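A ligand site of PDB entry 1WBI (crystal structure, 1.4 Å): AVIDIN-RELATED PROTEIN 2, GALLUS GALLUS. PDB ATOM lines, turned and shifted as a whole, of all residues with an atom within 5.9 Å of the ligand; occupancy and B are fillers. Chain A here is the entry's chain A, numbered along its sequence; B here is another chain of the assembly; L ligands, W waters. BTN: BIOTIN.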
ATOM      1  N   ASN A  15     -26.916   5.825  26.097  1.00  0.00           N
ATOM      2  CA  ASN A  15     -26.638   4.534  26.738  1.00  0.00           C
ATOM      3  C   ASN A  15     -25.878   4.631  28.009  1.00  0.00           C
ATOM      4  O   ASN A  15     -25.464   5.760  28.425  1.00  0.00           O
ATOM      5  CB  ASN A  15     -26.029   3.511  25.745  1.00  0.00           C
ATOM      6  CG  ASN A  15     -24.537   3.717  25.450  1.00  0.00           C
ATOM      7  OD1 ASN A  15     -23.807   4.407  26.173  1.00  0.00           O
ATOM      8  ND2 ASN A  15     -24.095   3.099  24.367  1.00  0.00           N
ATOM      9  N   LEU A  17     -22.910   3.871  28.881  1.00  0.00           N
ATOM     10  CA  LEU A  17     -21.533   4.352  28.867  1.00  0.00           C
ATOM     11  C   LEU A  17     -21.464   5.843  28.594  1.00  0.00           C
ATOM     12  O   LEU A  17     -20.366   6.385  28.483  1.00  0.00           O
ATOM     13  CB  LEU A  17     -20.696   3.619  27.835  1.00  0.00           C
ATOM     14  CG  LEU A  17     -20.436   2.155  28.154  1.00  0.00           C
ATOM     15  CD1 LEU A  17     -19.813   1.467  26.970  1.00  0.00           C
ATOM     16  CD2 LEU A  17     -19.513   1.950  29.390  1.00  0.00           C
ATOM     17  N   SER A  19     -22.716   7.247  25.815  1.00  0.00           N
ATOM     18  CA  SER A  19     -22.804   7.472  24.429  1.00  0.00           C
ATOM     19  C   SER A  19     -24.211   7.925  24.017  1.00  0.00           C
ATOM     20  O   SER A  19     -25.167   7.797  24.784  1.00  0.00           O
ATOM     21  CB  SER A  19     -22.421   6.209  23.633  1.00  0.00           C
ATOM     22  OG  SER A  19     -21.121   5.786  23.956  1.00  0.00           O
ATOM     23  N   TYR A  36     -23.719   8.154  15.558  1.00  0.00           N
ATOM     24  CA  TYR A  36     -23.312   7.667  16.855  1.00  0.00           C
ATOM     25  C   TYR A  36     -22.207   8.523  17.406  1.00  0.00           C
ATOM     26  O   TYR A  36     -21.206   8.754  16.717  1.00  0.00           O
ATOM     27  CB  TYR A  36     -22.797   6.202  16.728  1.00  0.00           C
ATOM     28  CG  TYR A  36     -22.930   5.383  17.995  1.00  0.00           C
ATOM     29  CD1 TYR A  36     -24.013   4.525  18.166  1.00  0.00           C
ATOM     30  CD2 TYR A  36     -22.001   5.475  19.017  1.00  0.00           C
ATOM     31  CE1 TYR A  36     -24.156   3.787  19.318  1.00  0.00           C
ATOM     32  CE2 TYR A  36     -22.120   4.715  20.179  1.00  0.00           C
ATOM     33  CZ  TYR A  36     -23.219   3.854  20.324  1.00  0.00           C
ATOM     34  OH  TYR A  36     -23.317   3.131  21.498  1.00  0.00           O
ATOM     35  N   THR A  38     -19.859   8.182  20.440  1.00  0.00           N
ATOM     36  CA  THR A  38     -19.391   7.396  21.560  1.00  0.00           C
ATOM     37  C   THR A  38     -18.747   8.286  22.622  1.00  0.00           C
ATOM     38  O   THR A  38     -18.124   9.319  22.270  1.00  0.00           O
ATOM     39  CB  THR A  38     -18.401   6.234  21.159  1.00  0.00           C
ATOM     40  OG1 THR A  38     -18.099   5.406  22.274  1.00  0.00           O
ATOM     41  CG2 THR A  38     -17.073   6.764  20.512  1.00  0.00           C
ATOM     42  N   ALA A  39     -18.929   7.887  23.881  1.00  0.00           N
ATOM     43  CA  ALA A  39     -18.262   8.530  25.036  1.00  0.00           C
ATOM     44  C   ALA A  39     -16.914   7.926  25.339  1.00  0.00           C
ATOM     45  O   ALA A  39     -16.134   8.489  26.136  1.00  0.00           O
ATOM     46  CB  ALA A  39     -19.130   8.395  26.274  1.00  0.00           C
ATOM     47  N   VAL A  40     -16.609   6.762  24.735  1.00  0.00           N
ATOM     48  CA  VAL A  40     -15.465   5.957  25.049  1.00  0.00           C
ATOM     49  C   VAL A  40     -14.855   5.384  23.772  1.00  0.00           C
ATOM     50  O   VAL A  40     -15.536   5.249  22.763  1.00  0.00           O
ATOM     51  CB  VAL A  40     -15.784   4.816  26.096  1.00  0.00           C
ATOM     52  CG1 VAL A  40     -16.385   5.380  27.392  1.00  0.00           C
ATOM     53  CG2 VAL A  40     -16.769   3.784  25.519  1.00  0.00           C
ATOM     54  N   ALA A  41     -13.569   5.051  23.808  1.00  0.00           N
ATOM     55  CA  ALA A  41     -12.846   4.530  22.649  1.00  0.00           C
ATOM     56  C   ALA A  41     -11.495   4.001  23.070  1.00  0.00           C
ATOM     57  O   ALA A  41     -11.025   4.282  24.181  1.00  0.00           O
ATOM     58  CB  ALA A  41     -12.687   5.639  21.543  1.00  0.00           C
ATOM     59  N   ASP A  42     -10.848   3.264  22.175  1.00  0.00           N
ATOM     60  CA  ASP A  42      -9.449   2.905  22.374  1.00  0.00           C
ATOM     61  C   ASP A  42      -8.560   4.149  22.480  1.00  0.00           C
ATOM     62  O   ASP A  42      -7.606   4.168  23.278  1.00  0.00           O
ATOM     63  CB  ASP A  42      -8.922   2.006  21.255  1.00  0.00           C
ATOM     64  CG  ASP A  42      -9.322   0.573  21.429  1.00  0.00           C
ATOM     65  OD1 ASP A  42      -8.933  -0.031  22.450  1.00  0.00           O
ATOM     66  OD2 ASP A  42     -10.022   0.032  20.564  1.00  0.00           O
ATOM     67  N   ASN A  43      -8.851   5.172  21.691  1.00  0.00           N
ATOM     68  CA  ASN A  43      -8.117   6.435  21.700  1.00  0.00           C
ATOM     69  C   ASN A  43      -9.141   7.561  21.805  1.00  0.00           C
ATOM     70  O   ASN A  43      -9.563   8.118  20.801  1.00  0.00           O
ATOM     71  CB  ASN A  43      -7.284   6.569  20.425  1.00  0.00           C
ATOM     72  CG  ASN A  43      -6.208   5.483  20.323  1.00  0.00           C
ATOM     73  OD1 ASN A  43      -5.164   5.580  20.971  1.00  0.00           O
ATOM     74  ND2 ASN A  43      -6.483   4.430  19.531  1.00  0.00           N
ATOM     75  N   TRP A  71     -16.702   3.466  12.478  1.00  0.00           N
ATOM     76  CA  TRP A  71     -16.013   4.508  13.245  1.00  0.00           C
ATOM     77  C   TRP A  71     -15.191   5.363  12.286  1.00  0.00           C
ATOM     78  O   TRP A  71     -14.386   4.869  11.524  1.00  0.00           O
ATOM     79  CB  TRP A  71     -15.153   3.890  14.337  1.00  0.00           C
ATOM     80  CG  TRP A  71     -15.996   3.075  15.298  1.00  0.00           C
ATOM     81  CD1 TRP A  71     -16.001   1.714  15.441  1.00  0.00           C
ATOM     82  CD2 TRP A  71     -17.016   3.561  16.169  1.00  0.00           C
ATOM     83  NE1 TRP A  71     -16.912   1.329  16.365  1.00  0.00           N
ATOM     84  CE2 TRP A  71     -17.557   2.445  16.837  1.00  0.00           C
ATOM     85  CE3 TRP A  71     -17.479   4.836  16.509  1.00  0.00           C
ATOM     86  CZ2 TRP A  71     -18.552   2.560  17.782  1.00  0.00           C
ATOM     87  CZ3 TRP A  71     -18.473   4.957  17.445  1.00  0.00           C
ATOM     88  CH2 TRP A  71     -19.006   3.827  18.081  1.00  0.00           C
ATOM     89  N   PHE A  73     -12.917   7.580  13.034  1.00  0.00           N
ATOM     90  CA  PHE A  73     -11.653   7.995  13.650  1.00  0.00           C
ATOM     91  C   PHE A  73     -10.677   6.824  13.943  1.00  0.00           C
ATOM     92  O   PHE A  73      -9.654   7.017  14.580  1.00  0.00           O
ATOM     93  CB  PHE A  73     -11.932   8.813  14.899  1.00  0.00           C
ATOM     94  CG  PHE A  73     -12.741   8.055  15.945  1.00  0.00           C
ATOM     95  CD1 PHE A  73     -12.097   7.336  16.920  1.00  0.00           C
ATOM     96  CD2 PHE A  73     -14.130   8.141  15.951  1.00  0.00           C
ATOM     97  CE1 PHE A  73     -12.828   6.635  17.861  1.00  0.00           C
ATOM     98  CE2 PHE A  73     -14.832   7.474  16.914  1.00  0.00           C
ATOM     99  CZ  PHE A  73     -14.176   6.733  17.852  1.00  0.00           C
ATOM    100  N   SER A  74     -11.060   5.595  13.546  1.00  0.00           N
ATOM    101  CA  SER A  74     -10.210   4.450  13.687  1.00  0.00           C
ATOM    102  C   SER A  74     -10.555   3.493  12.565  1.00  0.00           C
ATOM    103  O   SER A  74     -11.509   3.744  11.807  1.00  0.00           O
ATOM    104  CB  SER A  74     -10.398   3.758  15.034  1.00  0.00           C
ATOM    105  OG  SER A  74     -11.643   3.080  15.103  1.00  0.00           O
ATOM    106  N   GLU A  75      -9.809   2.392  12.518  1.00  0.00           N
ATOM    107  CA  GLU A  75     -10.111   1.308  11.564  1.00  0.00           C
ATOM    108  C   GLU A  75     -11.135   0.270  12.013  1.00  0.00           C
ATOM    109  O   GLU A  75     -11.431  -0.686  11.271  1.00  0.00           O
ATOM    110  CB  GLU A  75      -8.833   0.628  11.166  1.00  0.00           C
ATOM    111  CG  GLU A  75      -7.925   1.555  10.337  1.00  0.00           C
ATOM    112  CD  GLU A  75      -8.547   2.039   9.022  1.00  0.00           C
ATOM    113  OE1 GLU A  75      -9.418   1.399   8.376  1.00  0.00           O
ATOM    114  OE2 GLU A  75      -8.137   3.159   8.627  1.00  0.00           O
ATOM    115  N   SER A  76     -11.691   0.491  13.174  1.00  0.00           N
ATOM    116  CA  SER A  76     -12.656  -0.413  13.816  1.00  0.00           C
ATOM    117  C   SER A  76     -14.076  -0.306  13.243  1.00  0.00           C
ATOM    118  O   SER A  76     -14.457   0.727  12.661  1.00  0.00           O
ATOM    119  CB  SER A  76     -12.716  -0.079  15.330  1.00  0.00           C
ATOM    120  OG  SER A  76     -13.620  -0.889  16.092  1.00  0.00           O
ATOM    121  N   SER A  78     -18.093  -1.504  14.819  1.00  0.00           N
ATOM    122  CA  SER A  78     -18.912  -2.170  15.851  1.00  0.00           C
ATOM    123  C   SER A  78     -20.279  -2.553  15.301  1.00  0.00           C
ATOM    124  O   SER A  78     -20.777  -1.900  14.415  1.00  0.00           O
ATOM    125  CB  SER A  78     -19.116  -1.294  17.067  1.00  0.00           C
ATOM    126  OG  SER A  78     -17.862  -1.095  17.748  1.00  0.00           O
ATOM    127  N   PHE A  80     -24.239  -3.747  16.903  1.00  0.00           N
ATOM    128  CA  PHE A  80     -25.149  -3.857  18.038  1.00  0.00           C
ATOM    129  C   PHE A  80     -26.368  -4.643  17.625  1.00  0.00           C
ATOM    130  O   PHE A  80     -26.926  -4.421  16.548  1.00  0.00           O
ATOM    131  CB  PHE A  80     -25.601  -2.443  18.477  1.00  0.00           C
ATOM    132  CG  PHE A  80     -24.523  -1.551  19.074  1.00  0.00           C
ATOM    133  CD1 PHE A  80     -24.456  -1.361  20.416  1.00  0.00           C
ATOM    134  CD2 PHE A  80     -23.557  -0.963  18.268  1.00  0.00           C
ATOM    135  CE1 PHE A  80     -23.462  -0.519  20.968  1.00  0.00           C
ATOM    136  CE2 PHE A  80     -22.551  -0.148  18.849  1.00  0.00           C
ATOM    137  CZ  PHE A  80     -22.517   0.027  20.158  1.00  0.00           C
ATOM    138  N   TRP A  98     -23.147  -6.169  21.876  1.00  0.00           N
ATOM    139  CA  TRP A  98     -22.325  -5.660  20.803  1.00  0.00           C
ATOM    140  C   TRP A  98     -21.055  -6.437  20.652  1.00  0.00           C
ATOM    141  O   TRP A  98     -20.561  -7.087  21.610  1.00  0.00           O
ATOM    142  CB  TRP A  98     -22.034  -4.139  20.957  1.00  0.00           C
ATOM    143  CG  TRP A  98     -21.395  -3.690  22.248  1.00  0.00           C
ATOM    144  CD1 TRP A  98     -22.039  -3.059  23.276  1.00  0.00           C
ATOM    145  CD2 TRP A  98     -20.024  -3.808  22.635  1.00  0.00           C
ATOM    146  NE1 TRP A  98     -21.142  -2.790  24.292  1.00  0.00           N
ATOM    147  CE2 TRP A  98     -19.896  -3.221  23.910  1.00  0.00           C
ATOM    148  CE3 TRP A  98     -18.870  -4.277  21.989  1.00  0.00           C
ATOM    149  CZ2 TRP A  98     -18.645  -3.185  24.593  1.00  0.00           C
ATOM    150  CZ3 TRP A  98     -17.671  -4.221  22.650  1.00  0.00           C
ATOM    151  CH2 TRP A  98     -17.551  -3.666  23.952  1.00  0.00           C
ATOM    152  N   GLN A 100     -17.180  -5.408  18.931  1.00  0.00           N
ATOM    153  CA  GLN A 100     -16.306  -4.389  18.349  1.00  0.00           C
ATOM    154  C   GLN A 100     -15.151  -5.123  17.713  1.00  0.00           C
ATOM    155  O   GLN A 100     -14.420  -5.845  18.369  1.00  0.00           O
ATOM    156  CB  GLN A 100     -15.788  -3.384  19.375  1.00  0.00           C
ATOM    157  CG  GLN A 100     -14.877  -2.372  18.706  1.00  0.00           C
ATOM    158  CD  GLN A 100     -14.234  -1.393  19.647  1.00  0.00           C
ATOM    159  OE1 GLN A 100     -14.390  -1.513  20.847  1.00  0.00           O
ATOM    160  NE2 GLN A 100     -13.451  -0.451  19.097  1.00  0.00           N
ATOM    161  N   LEU A 102     -11.543  -4.937  15.950  1.00  0.00           N
ATOM    162  CA  LEU A 102     -10.300  -4.191  15.734  1.00  0.00           C
ATOM    163  C   LEU A 102      -9.622  -4.705  14.461  1.00  0.00           C
ATOM    164  O   LEU A 102      -9.768  -5.867  14.052  1.00  0.00           O
ATOM    165  CB  LEU A 102      -9.342  -4.368  16.906  1.00  0.00           C
ATOM    166  CG  LEU A 102      -9.861  -3.823  18.238  1.00  0.00           C
ATOM    167  CD1 LEU A 102      -8.940  -4.253  19.379  1.00  0.00           C
ATOM    168  CD2 LEU A 102      -9.954  -2.328  18.179  1.00  0.00           C
ATOM    169  N   ARG A 115     -13.873  -7.708  20.560  1.00  0.00           N
ATOM    170  CA  ARG A 115     -14.406  -7.475  21.872  1.00  0.00           C
ATOM    171  C   ARG A 115     -15.909  -7.661  21.894  1.00  0.00           C
ATOM    172  O   ARG A 115     -16.591  -7.408  20.894  1.00  0.00           O
ATOM    173  CB  ARG A 115     -14.195  -6.012  22.271  1.00  0.00           C
ATOM    174  CG  ARG A 115     -12.858  -5.548  22.576  1.00  0.00           C
ATOM    175  CD  ARG A 115     -12.992  -4.119  23.209  1.00  0.00           C
ATOM    176  NE  ARG A 115     -11.644  -3.698  23.333  1.00  0.00           N
ATOM    177  CZ  ARG A 115     -11.090  -2.676  22.724  1.00  0.00           C
ATOM    178  NH1 ARG A 115     -11.796  -1.851  21.956  1.00  0.00           N
ATOM    179  NH2 ARG A 115      -9.807  -2.478  22.931  1.00  0.00           N
ATOM    180  N   ASN A 118     -22.165  -5.187  26.236  1.00  0.00           N
ATOM    181  CA  ASN A 118     -23.585  -4.907  26.330  1.00  0.00           C
ATOM    182  C   ASN A 118     -23.814  -3.432  26.481  1.00  0.00           C
ATOM    183  O   ASN A 118     -22.951  -2.676  26.940  1.00  0.00           O
ATOM    184  CB  ASN A 118     -24.165  -5.646  27.533  1.00  0.00           C
ATOM    185  CG  ASN A 118     -23.402  -5.365  28.826  1.00  0.00           C
ATOM    186  OD1 ASN A 118     -22.400  -6.007  29.134  1.00  0.00           O
ATOM    187  ND2 ASN A 118     -23.897  -4.418  29.572  1.00  0.00           N
ATOM    188  N   ASN A 119     -25.025  -2.996  26.168  1.00  0.00           N
ATOM    189  CA  ASN A 119     -25.436  -1.632  26.435  1.00  0.00           C
ATOM    190  C   ASN A 119     -26.936  -1.577  26.527  1.00  0.00           C
ATOM    191  O   ASN A 119     -27.648  -2.190  25.711  1.00  0.00           O
ATOM    192  CB  ASN A 119     -25.015  -0.660  25.341  1.00  0.00           C
ATOM    193  CG  ASN A 119     -23.597  -0.116  25.486  1.00  0.00           C
ATOM    194  OD1 ASN A 119     -22.869  -0.166  24.542  1.00  0.00           O
ATOM    195  ND2 ASN A 119     -23.274   0.553  26.603  1.00  0.00           N
ATOM    196  N   PHE A 121     -29.992   1.225  26.180  1.00  0.00           N
ATOM    197  CA  PHE A 121     -30.290   2.574  25.692  1.00  0.00           C
ATOM    198  C   PHE A 121     -31.672   2.990  26.158  1.00  0.00           C
ATOM    199  O   PHE A 121     -32.602   2.174  26.169  1.00  0.00           O
ATOM    200  CB  PHE A 121     -30.281   2.667  24.176  1.00  0.00           C
ATOM    201  CG  PHE A 121     -28.940   2.392  23.503  1.00  0.00           C
ATOM    202  CD1 PHE A 121     -28.210   3.432  22.944  1.00  0.00           C
ATOM    203  CD2 PHE A 121     -28.431   1.104  23.405  1.00  0.00           C
ATOM    204  CE1 PHE A 121     -27.032   3.189  22.265  1.00  0.00           C
ATOM    205  CE2 PHE A 121     -27.266   0.851  22.755  1.00  0.00           C
ATOM    206  CZ  PHE A 121     -26.536   1.901  22.179  1.00  0.00           C
ATOM    207  N   TRP B 111     -15.751  -1.790  29.936  1.00  0.00           N
ATOM    208  CA  TRP B 111     -16.296  -2.097  28.629  1.00  0.00           C
ATOM    209  C   TRP B 111     -15.235  -2.643  27.661  1.00  0.00           C
ATOM    210  O   TRP B 111     -15.555  -3.342  26.691  1.00  0.00           O
ATOM    211  CB  TRP B 111     -16.992  -0.890  27.986  1.00  0.00           C
ATOM    212  CG  TRP B 111     -16.016   0.131  27.537  1.00  0.00           C
ATOM    213  CD1 TRP B 111     -15.425   1.074  28.347  1.00  0.00           C
ATOM    214  CD2 TRP B 111     -15.422   0.268  26.260  1.00  0.00           C
ATOM    215  NE1 TRP B 111     -14.542   1.820  27.616  1.00  0.00           N
ATOM    216  CE2 TRP B 111     -14.508   1.351  26.323  1.00  0.00           C
ATOM    217  CE3 TRP B 111     -15.584  -0.388  25.036  1.00  0.00           C
ATOM    218  CZ2 TRP B 111     -13.755   1.768  25.239  1.00  0.00           C
ATOM    219  CZ3 TRP B 111     -14.829   0.010  23.963  1.00  0.00           C
ATOM    220  CH2 TRP B 111     -13.923   1.102  24.067  1.00  0.00           C
HETATM  221  C11 BTN L   1     -12.830   2.815  18.740  1.00  0.00           C
HETATM  222  O11 BTN L   1     -11.894   2.840  17.872  1.00  0.00           O
HETATM  223  O12 BTN L   1     -12.533   2.548  19.939  1.00  0.00           O
HETATM  224  C10 BTN L   1     -14.208   3.115  18.256  1.00  0.00           C
HETATM  225  C9  BTN L   1     -15.216   3.348  19.358  1.00  0.00           C
HETATM  226  C8  BTN L   1     -15.736   2.041  19.989  1.00  0.00           C
HETATM  227  C7  BTN L   1     -16.818   2.363  21.027  1.00  0.00           C
HETATM  228  C2  BTN L   1     -17.522   1.124  21.662  1.00  0.00           C
HETATM  229  S1  BTN L   1     -18.687   0.343  20.625  1.00  0.00           S
HETATM  230  C6  BTN L   1     -19.253  -0.640  22.029  1.00  0.00           C
HETATM  231  C5  BTN L   1     -19.249   0.296  23.227  1.00  0.00           C
HETATM  232  N1  BTN L   1     -20.500   0.979  23.343  1.00  0.00           N
HETATM  233  C3  BTN L   1     -20.313   2.291  23.184  1.00  0.00           C
HETATM  234  O3  BTN L   1     -21.304   3.178  23.257  1.00  0.00           O
HETATM  235  N2  BTN L   1     -19.083   2.580  22.903  1.00  0.00           N
HETATM  236  C4  BTN L   1     -18.240   1.425  22.978  1.00  0.00           C
HETATM  237  O   HOH W   1     -10.155   0.851  17.990  1.00  0.00           O
HETATM  238  O   HOH W   2      -9.993   4.828  18.989  1.00  0.00           O
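The side-chain hydroxyl of Ser 74 is in hydrogen-bond range of an oxygen (O11) of the ligand (2.8 Å).
The side-chain amide oxygen of Asn 119 lies within hydrogen-bond range of a nitrogen (N1) of the ligand, 2.9 Å away.
N of Asp 42 lies within hydrogen-bond range of O12 of the ligand (2.9 Å).
OG of Ser 78 sits close to S1 of the ligand.
OH of Tyr 36 lies within hydrogen-bond range of O3 of the ligand (2.7 Å).
An oxygen (O12) of the ligand is in hydrogen-bond range of the side-chain amide nitrogen (NE2) of Gln 100 (3.2 Å).
O3 of the ligand lies within hydrogen-bond range of ND2 of Asn 15, at 3.0 Å.
The side-chain hydroxyl (OG) of Ser 19 sits at hydrogen-bond distance from an oxygen (O3) of the ligand, at 2.7 Å.
A nitrogen (N2) of the ligand sits at hydrogen-bond distance from the side-chain hydroxyl of Thr 38, at 3.1 Å.
The indole nitrogen (NE1) of Trp 98 sits at hydrogen-bond distance from the side-chain amide oxygen (OD1) of Asn 119 (3.2 Å).
OD1 of Asn 15 sits at hydrogen-bond distance from N of Leu 17 (2.9 Å).
The side-chain amide nitrogen (NE2) of Gln 100 is in hydrogen-bond range of the side-chain hydroxyl (OG) of Ser 76, at 3.0 Å.
The side-chain hydroxyl of Thr 38 lies within hydrogen-bond range of the backbone carbonyl oxygen of Val 40 (2.6 Å).
The side-chain hydroxyl of Ser 78 sits at hydrogen-bond distance from the indole nitrogen of Trp 71 (2.9 Å).
N of Ser 76 sits at hydrogen-bond distance from OG of Ser 74 (3.2 Å).
NH1 of Arg 115 is in hydrogen-bond range of OE1 of Gln 100.
OG of Ser 19 sits at hydrogen-bond distance from N of Ala 39 (3.0 Å).
Leu 17 touches the ligand (CD1 to N1, 3.7 Å).
O of Val 40 touches C7 of the ligand, 3.6 Å away.
CA of Ala 41 touches O12 of the ligand (3.4 Å).
Trp 71 touches the ligand (CG to C10, 3.5 Å).
Phe 73 touches the ligand (CZ to C10, 3.6 Å).
Ser 76 touches the ligand (CB to O11, 3.96 Å).
Phe 80 touches the ligand.
Trp 98 touches the ligand (CE2 to C6, 3.3 Å).
Trp 111 of chain B touches the ligand (CZ3 to C2, 3.7 Å).
Hydrophobic or aromatic side chains that line the ligand: Leu 17, Tyr 36, Val 40, Ala 41, Trp 71, Phe 73, Phe 80, Trp 98 and Trp 111 of chain B.
18 residues have an atom within 4 Å of the ligand: Asn 15, Leu 17, Ser 19, Tyr 36, Thr 38, Val 40, Ala 41, Asp 42, Trp 71, Phe 73, Ser 74, Ser 76, Ser 78, Phe 80, Trp 98, Gln 100, Asn 119 and Trp 111 of chain B.
The nearest printed residue that does not touch the ligand is Asn 43 (4.8 Å).
Water W1 lies within hydrogen-bond range of an oxygen (O11) of the ligand and the side-chain carboxylate (OD2) of Asp 42.
Water W2 bridges N of Asn 43 and O11 of the ligand.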
